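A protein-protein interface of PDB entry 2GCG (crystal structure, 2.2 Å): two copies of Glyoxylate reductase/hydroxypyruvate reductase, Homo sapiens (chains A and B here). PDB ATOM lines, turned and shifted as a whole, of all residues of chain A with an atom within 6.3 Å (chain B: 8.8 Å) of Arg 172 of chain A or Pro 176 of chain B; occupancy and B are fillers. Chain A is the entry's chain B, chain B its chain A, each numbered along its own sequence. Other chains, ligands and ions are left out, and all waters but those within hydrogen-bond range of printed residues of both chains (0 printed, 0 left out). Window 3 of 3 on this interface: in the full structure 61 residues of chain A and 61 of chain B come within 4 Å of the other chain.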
ATOM      1  N   THR A 110      28.875  -5.714  17.197  1.00  0.00           N
ATOM      2  CA  THR A 110      28.428  -7.058  17.624  1.00  0.00           C
ATOM      3  C   THR A 110      26.906  -7.032  17.804  1.00  0.00           C
ATOM      4  O   THR A 110      26.192  -7.952  17.350  1.00  0.00           O
ATOM      5  CB  THR A 110      29.174  -7.538  18.894  1.00  0.00           C
ATOM      6  OG1 THR A 110      30.524  -7.820  18.544  1.00  0.00           O
ATOM      7  CG2 THR A 110      28.572  -8.811  19.467  1.00  0.00           C
ATOM      8  N   ASP A 111      26.400  -5.981  18.440  1.00  0.00           N
ATOM      9  CA  ASP A 111      24.982  -5.970  18.825  1.00  0.00           C
ATOM     10  C   ASP A 111      24.085  -5.778  17.578  1.00  0.00           C
ATOM     11  O   ASP A 111      23.104  -6.484  17.399  1.00  0.00           O
ATOM     12  CB  ASP A 111      24.681  -4.872  19.838  1.00  0.00           C
ATOM     13  CG  ASP A 111      25.079  -5.226  21.244  1.00  0.00           C
ATOM     14  OD1 ASP A 111      25.622  -4.312  21.916  1.00  0.00           O
ATOM     15  OD2 ASP A 111      24.862  -6.389  21.695  1.00  0.00           O
ATOM     16  N   ARG A 165      31.723 -13.704  19.465  1.00  0.00           N
ATOM     17  CA  ARG A 165      31.102 -12.479  19.965  1.00  0.00           C
ATOM     18  C   ARG A 165      29.678 -12.359  19.485  1.00  0.00           C
ATOM     19  O   ARG A 165      28.740 -12.184  20.279  1.00  0.00           O
ATOM     20  CB  ARG A 165      31.915 -11.238  19.550  1.00  0.00           C
ATOM     21  CG  ARG A 165      33.243 -11.067  20.332  1.00  0.00           C
ATOM     22  CD  ARG A 165      34.133  -9.908  19.805  1.00  0.00           C
ATOM     23  NE  ARG A 165      34.706 -10.150  18.467  1.00  0.00           N
ATOM     24  CZ  ARG A 165      35.950 -10.584  18.241  1.00  0.00           C
ATOM     25  NH1 ARG A 165      36.761 -10.822  19.261  1.00  0.00           N
ATOM     26  NH2 ARG A 165      36.391 -10.778  16.988  1.00  0.00           N
ATOM     27  N   GLY A 167      27.788 -14.731  17.511  1.00  0.00           N
ATOM     28  CA  GLY A 167      27.020 -15.932  17.905  1.00  0.00           C
ATOM     29  C   GLY A 167      26.452 -15.890  19.321  1.00  0.00           C
ATOM     30  O   GLY A 167      25.326 -16.359  19.553  1.00  0.00           O
ATOM     31  N   GLN A 168      27.211 -15.298  20.258  1.00  0.00           N
ATOM     32  CA  GLN A 168      26.753 -15.083  21.652  1.00  0.00           C
ATOM     33  C   GLN A 168      25.623 -14.022  21.782  1.00  0.00           C
ATOM     34  O   GLN A 168      24.628 -14.254  22.463  1.00  0.00           O
ATOM     35  CB  GLN A 168      27.947 -14.701  22.557  1.00  0.00           C
ATOM     36  CG  GLN A 168      28.903 -15.874  22.908  1.00  0.00           C
ATOM     37  CD  GLN A 168      30.328 -15.430  23.310  1.00  0.00           C
ATOM     38  OE1 GLN A 168      30.506 -14.463  24.051  1.00  0.00           O
ATOM     39  NE2 GLN A 168      31.347 -16.159  22.830  1.00  0.00           N
ATOM     40  N   ALA A 169      25.807 -12.866  21.118  1.00  0.00           N
ATOM     41  CA  ALA A 169      24.796 -11.829  21.049  1.00  0.00           C
ATOM     42  C   ALA A 169      23.509 -12.265  20.353  1.00  0.00           C
ATOM     43  O   ALA A 169      22.447 -11.748  20.668  1.00  0.00           O
ATOM     44  CB  ALA A 169      25.349 -10.611  20.433  1.00  0.00           C
ATOM     45  N   ILE A 170      23.628 -13.221  19.429  1.00  0.00           N
ATOM     46  CA  ILE A 170      22.516 -13.893  18.745  1.00  0.00           C
ATOM     47  C   ILE A 170      21.721 -14.792  19.706  1.00  0.00           C
ATOM     48  O   ILE A 170      20.494 -14.597  19.894  1.00  0.00           O
ATOM     49  CB  ILE A 170      23.034 -14.704  17.456  1.00  0.00           C
ATOM     50  CG1 ILE A 170      23.452 -13.733  16.351  1.00  0.00           C
ATOM     51  CG2 ILE A 170      21.963 -15.628  16.915  1.00  0.00           C
ATOM     52  CD1 ILE A 170      24.084 -14.356  15.126  1.00  0.00           C
ATOM     53  N   ALA A 171      22.409 -15.760  20.335  1.00  0.00           N
ATOM     54  CA  ALA A 171      21.784 -16.659  21.308  1.00  0.00           C
ATOM     55  C   ALA A 171      21.077 -15.885  22.420  1.00  0.00           C
ATOM     56  O   ALA A 171      20.040 -16.309  22.930  1.00  0.00           O
ATOM     57  CB  ALA A 171      22.826 -17.574  21.910  1.00  0.00           C
ATOM     58  N   ARG A 172      21.636 -14.734  22.789  1.00  0.00           N
ATOM     59  CA  ARG A 172      21.159 -13.993  23.957  1.00  0.00           C
ATOM     60  C   ARG A 172      19.827 -13.382  23.560  1.00  0.00           C
ATOM     61  O   ARG A 172      18.881 -13.335  24.362  1.00  0.00           O
ATOM     62  CB  ARG A 172      22.236 -12.953  24.332  1.00  0.00           C
ATOM     63  CG  ARG A 172      22.023 -12.061  25.535  1.00  0.00           C
ATOM     64  CD  ARG A 172      23.261 -11.131  25.715  1.00  0.00           C
ATOM     65  NE  ARG A 172      24.436 -11.924  26.082  1.00  0.00           N
ATOM     66  CZ  ARG A 172      25.583 -11.924  25.411  1.00  0.00           C
ATOM     67  NH1 ARG A 172      25.771 -11.115  24.366  1.00  0.00           N
ATOM     68  NH2 ARG A 172      26.559 -12.724  25.798  1.00  0.00           N
ATOM     69  N   ARG A 173      19.758 -12.938  22.297  1.00  0.00           N
ATOM     70  CA  ARG A 173      18.529 -12.382  21.712  1.00  0.00           C
ATOM     71  C   ARG A 173      17.493 -13.486  21.419  1.00  0.00           C
ATOM     72  O   ARG A 173      16.317 -13.230  21.466  1.00  0.00           O
ATOM     73  CB  ARG A 173      18.862 -11.565  20.471  1.00  0.00           C
ATOM     74  CG  ARG A 173      19.427 -10.210  20.800  1.00  0.00           C
ATOM     75  CD  ARG A 173      20.406  -9.688  19.768  1.00  0.00           C
ATOM     76  NE  ARG A 173      20.114  -8.299  19.445  1.00  0.00           N
ATOM     77  CZ  ARG A 173      20.715  -7.201  19.922  1.00  0.00           C
ATOM     78  NH1 ARG A 173      21.782  -7.295  20.779  1.00  0.00           N
ATOM     79  NH2 ARG A 173      20.209  -5.975  19.520  1.00  0.00           N
ATOM     80  N   LEU A 174      17.945 -14.716  21.165  1.00  0.00           N
ATOM     81  CA  LEU A 174      17.052 -15.844  20.842  1.00  0.00           C
ATOM     82  C   LEU A 174      16.373 -16.523  22.042  1.00  0.00           C
ATOM     83  O   LEU A 174      15.233 -17.010  21.929  1.00  0.00           O
ATOM     84  CB  LEU A 174      17.823 -16.890  20.050  1.00  0.00           C
ATOM     85  CG  LEU A 174      17.568 -17.070  18.552  1.00  0.00           C
ATOM     86  CD1 LEU A 174      16.780 -15.896  17.885  1.00  0.00           C
ATOM     87  CD2 LEU A 174      18.845 -17.529  17.730  1.00  0.00           C
ATOM     88  N   LYS A 175      17.091 -16.545  23.174  1.00  0.00           N
ATOM     89  CA  LYS A 175      16.658 -17.152  24.447  1.00  0.00           C
ATOM     90  C   LYS A 175      15.189 -16.858  24.926  1.00  0.00           C
ATOM     91  O   LYS A 175      14.486 -17.787  25.292  1.00  0.00           O
ATOM     92  CB  LYS A 175      17.702 -16.767  25.541  1.00  0.00           C
ATOM     93  CG  LYS A 175      17.491 -17.338  26.956  1.00  0.00           C
ATOM     94  CD  LYS A 175      18.800 -17.365  27.790  1.00  0.00           C
ATOM     95  CE  LYS A 175      18.645 -18.226  29.037  1.00  0.00           C
ATOM     96  NZ  LYS A 175      19.891 -18.999  29.314  1.00  0.00           N
ATOM     97  N   PRO A 176      14.747 -15.569  24.999  1.00  0.00           N
ATOM     98  CA  PRO A 176      13.363 -15.334  25.479  1.00  0.00           C
ATOM     99  C   PRO A 176      12.245 -15.708  24.479  1.00  0.00           C
ATOM    100  O   PRO A 176      11.086 -15.656  24.848  1.00  0.00           O
ATOM    101  CB  PRO A 176      13.329 -13.828  25.755  1.00  0.00           C
ATOM    102  CG  PRO A 176      14.384 -13.282  24.827  1.00  0.00           C
ATOM    103  CD  PRO A 176      15.462 -14.303  24.751  1.00  0.00           C
ATOM    104  N   PHE A 177      12.605 -16.116  23.262  1.00  0.00           N
ATOM    105  CA  PHE A 177      11.664 -16.649  22.318  1.00  0.00           C
ATOM    106  C   PHE A 177      11.273 -18.081  22.706  1.00  0.00           C
ATOM    107  O   PHE A 177      10.571 -18.744  21.989  1.00  0.00           O
ATOM    108  CB  PHE A 177      12.254 -16.611  20.921  1.00  0.00           C
ATOM    109  CG  PHE A 177      12.325 -15.226  20.321  1.00  0.00           C
ATOM    110  CD1 PHE A 177      13.356 -14.353  20.662  1.00  0.00           C
ATOM    111  CD2 PHE A 177      11.353 -14.797  19.409  1.00  0.00           C
ATOM    112  CE1 PHE A 177      13.421 -13.079  20.103  1.00  0.00           C
ATOM    113  CE2 PHE A 177      11.393 -13.556  18.849  1.00  0.00           C
ATOM    114  CZ  PHE A 177      12.426 -12.678  19.183  1.00  0.00           C
ATOM    115  N   PHE A 182      20.123 -24.987  23.106  1.00  0.00           N
ATOM    116  CA  PHE A 182      21.169 -24.425  22.210  1.00  0.00           C
ATOM    117  C   PHE A 182      22.315 -25.409  22.057  1.00  0.00           C
ATOM    118  O   PHE A 182      22.835 -25.948  23.041  1.00  0.00           O
ATOM    119  CB  PHE A 182      21.812 -23.119  22.728  1.00  0.00           C
ATOM    120  CG  PHE A 182      20.895 -21.949  22.794  1.00  0.00           C
ATOM    121  CD1 PHE A 182      20.160 -21.694  23.973  1.00  0.00           C
ATOM    122  CD2 PHE A 182      20.793 -21.052  21.711  1.00  0.00           C
ATOM    123  CE1 PHE A 182      19.334 -20.598  24.063  1.00  0.00           C
ATOM    124  CE2 PHE A 182      19.955 -19.948  21.777  1.00  0.00           C
ATOM    125  CZ  PHE A 182      19.229 -19.700  22.961  1.00  0.00           C
ATOM    126  N   GLU A 196      26.188 -19.360  29.526  1.00  0.00           N
ATOM    127  CA  GLU A 196      25.115 -18.384  29.590  1.00  0.00           C
ATOM    128  C   GLU A 196      23.822 -18.961  28.964  1.00  0.00           C
ATOM    129  O   GLU A 196      22.696 -18.629  29.377  1.00  0.00           O
ATOM    130  CB  GLU A 196      25.542 -17.050  28.944  1.00  0.00           C
ATOM    131  CG  GLU A 196      24.439 -15.976  28.973  1.00  0.00           C
ATOM    132  CD  GLU A 196      24.819 -14.669  28.299  1.00  0.00           C
ATOM    133  OE1 GLU A 196      26.009 -14.491  27.883  1.00  0.00           O
ATOM    134  OE2 GLU A 196      23.902 -13.818  28.176  1.00  0.00           O
ATOM    135  N   PHE A 197      23.999 -19.860  28.002  1.00  0.00           N
ATOM    136  CA  PHE A 197      22.891 -20.392  27.211  1.00  0.00           C
ATOM    137  C   PHE A 197      22.628 -21.882  27.528  1.00  0.00           C
ATOM    138  O   PHE A 197      21.753 -22.501  26.916  1.00  0.00           O
ATOM    139  CB  PHE A 197      23.172 -20.126  25.716  1.00  0.00           C
ATOM    140  CG  PHE A 197      23.682 -18.710  25.457  1.00  0.00           C
ATOM    141  CD1 PHE A 197      25.015 -18.468  25.129  1.00  0.00           C
ATOM    142  CD2 PHE A 197      22.878 -17.631  25.644  1.00  0.00           C
ATOM    143  CE1 PHE A 197      25.496 -17.159  24.982  1.00  0.00           C
ATOM    144  CE2 PHE A 197      23.355 -16.333  25.457  1.00  0.00           C
ATOM    145  CZ  PHE A 197      24.655 -16.113  25.151  1.00  0.00           C
ATOM    146  N   VAL B 118       7.590  -8.982  17.123  1.00  0.00           N
ATOM    147  CA  VAL B 118       9.017  -8.664  17.085  1.00  0.00           C
ATOM    148  C   VAL B 118       9.566  -8.909  15.657  1.00  0.00           C
ATOM    149  O   VAL B 118      10.275  -8.052  15.135  1.00  0.00           O
ATOM    150  CB  VAL B 118       9.786  -9.314  18.267  1.00  0.00           C
ATOM    151  CG1 VAL B 118      11.241  -9.058  18.179  1.00  0.00           C
ATOM    152  CG2 VAL B 118       9.233  -8.760  19.595  1.00  0.00           C
ATOM    153  N   LEU B 153      17.802  -1.218  18.190  1.00  0.00           N
ATOM    154  CA  LEU B 153      17.151  -1.341  19.512  1.00  0.00           C
ATOM    155  C   LEU B 153      18.086  -1.080  20.719  1.00  0.00           C
ATOM    156  O   LEU B 153      17.610  -1.019  21.880  1.00  0.00           O
ATOM    157  CB  LEU B 153      16.531  -2.727  19.688  1.00  0.00           C
ATOM    158  CG  LEU B 153      15.059  -3.154  19.516  1.00  0.00           C
ATOM    159  CD1 LEU B 153      14.036  -2.102  19.825  1.00  0.00           C
ATOM    160  CD2 LEU B 153      14.764  -3.764  18.191  1.00  0.00           C
ATOM    161  N   THR B 154      19.396  -0.949  20.466  1.00  0.00           N
ATOM    162  CA  THR B 154      20.347  -0.764  21.575  1.00  0.00           C
ATOM    163  C   THR B 154      20.212   0.643  22.197  1.00  0.00           C
ATOM    164  O   THR B 154      20.206   1.647  21.475  1.00  0.00           O
ATOM    165  CB  THR B 154      21.820  -1.187  21.212  1.00  0.00           C
ATOM    166  OG1 THR B 154      21.861  -2.605  20.852  1.00  0.00           O
ATOM    167  CG2 THR B 154      22.739  -0.998  22.408  1.00  0.00           C
ATOM    168  N   ALA B 169       4.859 -10.358  26.803  1.00  0.00           N
ATOM    169  CA  ALA B 169       5.653 -11.277  25.961  1.00  0.00           C
ATOM    170  C   ALA B 169       6.487 -10.623  24.857  1.00  0.00           C
ATOM    171  O   ALA B 169       7.453 -11.224  24.394  1.00  0.00           O
ATOM    172  CB  ALA B 169       4.744 -12.354  25.341  1.00  0.00           C
ATOM    173  N   ILE B 170       6.100  -9.413  24.436  1.00  0.00           N
ATOM    174  CA  ILE B 170       6.820  -8.686  23.418  1.00  0.00           C
ATOM    175  C   ILE B 170       7.969  -7.994  24.076  1.00  0.00           C
ATOM    176  O   ILE B 170       9.088  -8.075  23.552  1.00  0.00           O
ATOM    177  CB  ILE B 170       5.947  -7.646  22.683  1.00  0.00           C
ATOM    178  CG1 ILE B 170       4.951  -8.340  21.709  1.00  0.00           C
ATOM    179  CG2 ILE B 170       6.827  -6.683  21.919  1.00  0.00           C
ATOM    180  CD1 ILE B 170       3.745  -7.463  21.327  1.00  0.00           C
ATOM    181  N   ALA B 171       7.694  -7.339  25.229  1.00  0.00           N
ATOM    182  CA  ALA B 171       8.727  -6.683  26.048  1.00  0.00           C
ATOM    183  C   ALA B 171       9.856  -7.640  26.458  1.00  0.00           C
ATOM    184  O   ALA B 171      11.043  -7.349  26.293  1.00  0.00           O
ATOM    185  CB  ALA B 171       8.102  -5.976  27.280  1.00  0.00           C
ATOM    186  N   ARG B 172       9.445  -8.809  26.923  1.00  0.00           N
ATOM    187  CA  ARG B 172      10.314  -9.892  27.304  1.00  0.00           C
ATOM    188  C   ARG B 172      11.209 -10.307  26.118  1.00  0.00           C
ATOM    189  O   ARG B 172      12.354 -10.672  26.313  1.00  0.00           O
ATOM    190  CB  ARG B 172       9.413 -11.052  27.780  1.00  0.00           C
ATOM    191  CG  ARG B 172      10.090 -12.154  28.517  1.00  0.00           C
ATOM    192  CD  ARG B 172       9.206 -12.728  29.646  1.00  0.00           C
ATOM    193  NE  ARG B 172       8.020 -13.387  29.127  1.00  0.00           N
ATOM    194  CZ  ARG B 172       6.765 -13.121  29.486  1.00  0.00           C
ATOM    195  NH1 ARG B 172       6.489 -12.218  30.429  1.00  0.00           N
ATOM    196  NH2 ARG B 172       5.779 -13.789  28.904  1.00  0.00           N
ATOM    197  N   ARG B 173      10.683 -10.244  24.886  1.00  0.00           N
ATOM    198  CA  ARG B 173      11.449 -10.662  23.708  1.00  0.00           C
ATOM    199  C   ARG B 173      12.393  -9.543  23.206  1.00  0.00           C
ATOM    200  O   ARG B 173      13.411  -9.827  22.536  1.00  0.00           O
ATOM    201  CB  ARG B 173      10.499 -11.087  22.581  1.00  0.00           C
ATOM    202  CG  ARG B 173      10.174 -12.586  22.564  1.00  0.00           C
ATOM    203  CD  ARG B 173       8.905 -12.911  21.762  1.00  0.00           C
ATOM    204  NE  ARG B 173       8.603 -14.350  21.931  1.00  0.00           N
ATOM    205  CZ  ARG B 173       8.025 -14.865  23.021  1.00  0.00           C
ATOM    206  NH1 ARG B 173       7.637 -14.056  24.001  1.00  0.00           N
ATOM    207  NH2 ARG B 173       7.819 -16.167  23.143  1.00  0.00           N
ATOM    208  N   LEU B 174      12.045  -8.292  23.510  1.00  0.00           N
ATOM    209  CA  LEU B 174      12.854  -7.123  23.100  1.00  0.00           C
ATOM    210  C   LEU B 174      13.949  -6.754  24.129  1.00  0.00           C
ATOM    211  O   LEU B 174      14.965  -6.140  23.778  1.00  0.00           O
ATOM    212  CB  LEU B 174      11.950  -5.911  22.904  1.00  0.00           C
ATOM    213  CG  LEU B 174      11.336  -5.433  21.590  1.00  0.00           C
ATOM    214  CD1 LEU B 174      11.670  -6.265  20.362  1.00  0.00           C
ATOM    215  CD2 LEU B 174       9.851  -5.116  21.755  1.00  0.00           C
ATOM    216  N   LYS B 175      13.751  -7.147  25.381  1.00  0.00           N
ATOM    217  CA  LYS B 175      14.696  -6.821  26.450  1.00  0.00           C
ATOM    218  C   LYS B 175      16.143  -7.178  26.058  1.00  0.00           C
ATOM    219  O   LYS B 175      16.984  -6.287  26.042  1.00  0.00           O
ATOM    220  CB  LYS B 175      14.270  -7.463  27.785  1.00  0.00           C
ATOM    221  CG  LYS B 175      15.010  -7.039  29.037  1.00  0.00           C
ATOM    222  CD  LYS B 175      14.306  -7.624  30.287  1.00  0.00           C
ATOM    223  CE  LYS B 175      15.184  -7.501  31.528  1.00  0.00           C
ATOM    224  NZ  LYS B 175      14.419  -7.720  32.797  1.00  0.00           N
ATOM    225  N   PRO B 176      16.431  -8.457  25.699  1.00  0.00           N
ATOM    226  CA  PRO B 176      17.837  -8.806  25.386  1.00  0.00           C
ATOM    227  C   PRO B 176      18.440  -8.091  24.178  1.00  0.00           C
ATOM    228  O   PRO B 176      19.662  -8.239  23.895  1.00  0.00           O
ATOM    229  CB  PRO B 176      17.770 -10.292  25.095  1.00  0.00           C
ATOM    230  CG  PRO B 176      16.294 -10.546  24.777  1.00  0.00           C
ATOM    231  CD  PRO B 176      15.549  -9.643  25.636  1.00  0.00           C
ATOM    232  N   PHE B 177      17.608  -7.320  23.470  1.00  0.00           N
ATOM    233  CA  PHE B 177      18.097  -6.493  22.347  1.00  0.00           C
ATOM    234  C   PHE B 177      18.783  -5.199  22.839  1.00  0.00           C
ATOM    235  O   PHE B 177      19.244  -4.379  22.042  1.00  0.00           O
ATOM    236  CB  PHE B 177      16.976  -6.215  21.324  1.00  0.00           C
ATOM    237  CG  PHE B 177      16.584  -7.434  20.504  1.00  0.00           C
ATOM    238  CD1 PHE B 177      15.721  -8.398  21.016  1.00  0.00           C
ATOM    239  CD2 PHE B 177      17.078  -7.606  19.220  1.00  0.00           C
ATOM    240  CE1 PHE B 177      15.359  -9.504  20.264  1.00  0.00           C
ATOM    241  CE2 PHE B 177      16.729  -8.722  18.469  1.00  0.00           C
ATOM    242  CZ  PHE B 177      15.876  -9.676  19.004  1.00  0.00           C
ATOM    243  N   GLY B 178      18.838  -5.007  24.157  1.00  0.00           N
ATOM    244  CA  GLY B 178      19.574  -3.863  24.701  1.00  0.00           C
ATOM    245  C   GLY B 178      18.706  -2.639  24.954  1.00  0.00           C
ATOM    246  O   GLY B 178      19.230  -1.536  25.197  1.00  0.00           O
ATOM    247  N   VAL B 179      17.377  -2.833  24.879  1.00  0.00           N
ATOM    248  CA  VAL B 179      16.405  -1.786  25.253  1.00  0.00           C
ATOM    249  C   VAL B 179      16.738  -1.185  26.624  1.00  0.00           C
ATOM    250  O   VAL B 179      16.910  -1.901  27.609  1.00  0.00           O
ATOM    251  CB  VAL B 179      14.949  -2.321  25.290  1.00  0.00           C
ATOM    252  CG1 VAL B 179      13.991  -1.305  25.926  1.00  0.00           C
ATOM    253  CG2 VAL B 179      14.486  -2.692  23.885  1.00  0.00           C
ATOM    254  N   GLN B 180      16.819   0.140  26.673  1.00  0.00           N
ATOM    255  CA  GLN B 180      17.174   0.851  27.884  1.00  0.00           C
ATOM    256  C   GLN B 180      15.987   1.085  28.820  1.00  0.00           C
ATOM    257  O   GLN B 180      16.157   1.103  30.051  1.00  0.00           O
ATOM    258  CB  GLN B 180      17.745   2.194  27.515  1.00  0.00           C
ATOM    259  CG  GLN B 180      18.526   2.824  28.641  1.00  0.00           C
ATOM    260  CD  GLN B 180      18.941   4.242  28.330  1.00  0.00           C
ATOM    261  OE1 GLN B 180      20.122   4.513  28.094  1.00  0.00           O
ATOM    262  NE2 GLN B 180      17.967   5.163  28.315  1.00  0.00           N
ATOM    263  N   PHE B 182      11.524   0.711  29.141  1.00  0.00           N
ATOM    264  CA  PHE B 182      10.173   0.306  28.735  1.00  0.00           C
ATOM    265  C   PHE B 182       9.074   1.223  29.325  1.00  0.00           C
ATOM    266  O   PHE B 182       8.978   1.385  30.542  1.00  0.00           O
ATOM    267  CB  PHE B 182       9.925  -1.141  29.164  1.00  0.00           C
ATOM    268  CG  PHE B 182      10.653  -2.144  28.333  1.00  0.00           C
ATOM    269  CD1 PHE B 182      11.746  -2.847  28.858  1.00  0.00           C
ATOM    270  CD2 PHE B 182      10.229  -2.408  27.030  1.00  0.00           C
ATOM    271  CE1 PHE B 182      12.413  -3.797  28.084  1.00  0.00           C
ATOM    272  CE2 PHE B 182      10.892  -3.334  26.240  1.00  0.00           C
ATOM    273  CZ  PHE B 182      11.980  -4.043  26.766  1.00  0.00           C
ATOM    274  N   PHE B 197       9.996  -5.761  33.670  1.00  0.00           N
ATOM    275  CA  PHE B 197      10.686  -4.938  32.674  1.00  0.00           C
ATOM    276  C   PHE B 197      11.082  -3.594  33.246  1.00  0.00           C
ATOM    277  O   PHE B 197      11.663  -2.765  32.548  1.00  0.00           O
ATOM    278  CB  PHE B 197       9.829  -4.758  31.418  1.00  0.00           C
ATOM    279  CG  PHE B 197       9.076  -5.997  31.024  1.00  0.00           C
ATOM    280  CD1 PHE B 197       7.686  -6.031  31.108  1.00  0.00           C
ATOM    281  CD2 PHE B 197       9.754  -7.130  30.610  1.00  0.00           C
ATOM    282  CE1 PHE B 197       6.988  -7.171  30.774  1.00  0.00           C
ATOM    283  CE2 PHE B 197       9.065  -8.269  30.271  1.00  0.00           C
ATOM    284  CZ  PHE B 197       7.688  -8.302  30.359  1.00  0.00           C
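The backbone carbonyl oxygen (O) of Phe 177 of chain B is in hydrogen-bond range of the guanidinium group (NH2) of Arg 173 of chain A (3.1 Å).
The backbone carbonyl oxygen (O) of Phe 177 of chain B is in hydrogen-bond range of the side-chain hydroxyl (OG1) of Thr 154 of chain B (3.4 Å).
O of Ala 169 of chain B lies within hydrogen-bond range of NH1 of Arg 173 of chain B (2.9 Å).
OD2 of Asp 111 of chain A is in salt-bridge range of NH1 of Arg 173 of chain A, at 3.3 Å.
NH2 of Arg 172 of chain A is in salt-bridge range of OE1 of Glu 196 of chain A (2.8 Å).
Among the printed residues, merely in contact across the chains: Arg 172 of chain A with Pro 176 of chain B, Pro 176 of chain A with Pro 176 of chain B, Pro 176 of chain A with Arg 172 of chain B, Pro 176 of chain A with Arg 173 of chain B, Arg 173 of chain A with Pro 176 of chain B, Asp 111 of chain A with Thr 154 of chain B, Phe 177 of chain A with Arg 173 of chain B, Phe 177 of chain A with Val 118 of chain B and Arg 173 of chain A with Thr 154 of chain B.
Printed residues of chain B within 4 Å of Asp 111 of chain A: Thr 154.
Ala 169 of chain A touches none of the printed residues of chain B.
Arg 172 of chain A touches one residue of chain B.
Of the printed residues of chain B, Phe 177 of chain A touches Val 118 and Arg 173.
Printed residues of chain A within 4 Å of Pro 176 of chain B: Arg 172 (3.3 Å), Arg 173 (3.7 Å) and Pro 176 (3.3 Å).
The nearest residue of chain B that does not touch Arg 172 of chain A is Phe 177 of chain B (6.2 Å).
The nearest printed residue of chain A that does not touch Phe 177 of chain B is Phe 177 of chain A (4.1 Å).
Of the 17 printed residues of chain B, 6 touch a printed residue of chain A.
Hydrophobic or aromatic side chains of chain B that line the printed part of chain A: Val 118, Pro 176 and Phe 177.
Of the 17 printed residues of chain A, 5 touch a printed residue of chain B.
Among the printed residues, no Asp or Glu carboxylate lies within 4 Å of a Lys or Arg side-chain nitrogen of the other chain.
Arg 172 of chain A touches Pro 176 of chain B, and with the chains exchanged Pro 176 of chain A touches Arg 172 of chain B.
Arg 173 of chain A touches Pro 176 of chain B, and with the chains exchanged Pro 176 of chain A touches Arg 173 of chain B.
Arg 173 of chain A touches Phe 177 of chain B, and with the chains exchanged Phe 177 of chain A touches Arg 173 of chain B.
Pro 176 of chain A touches its own counterpart, Pro 176 of chain B.
Positions printed for both chains: 169, 170, 171, 172, 173, 174, 175, 176, 177, 182 and 197.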
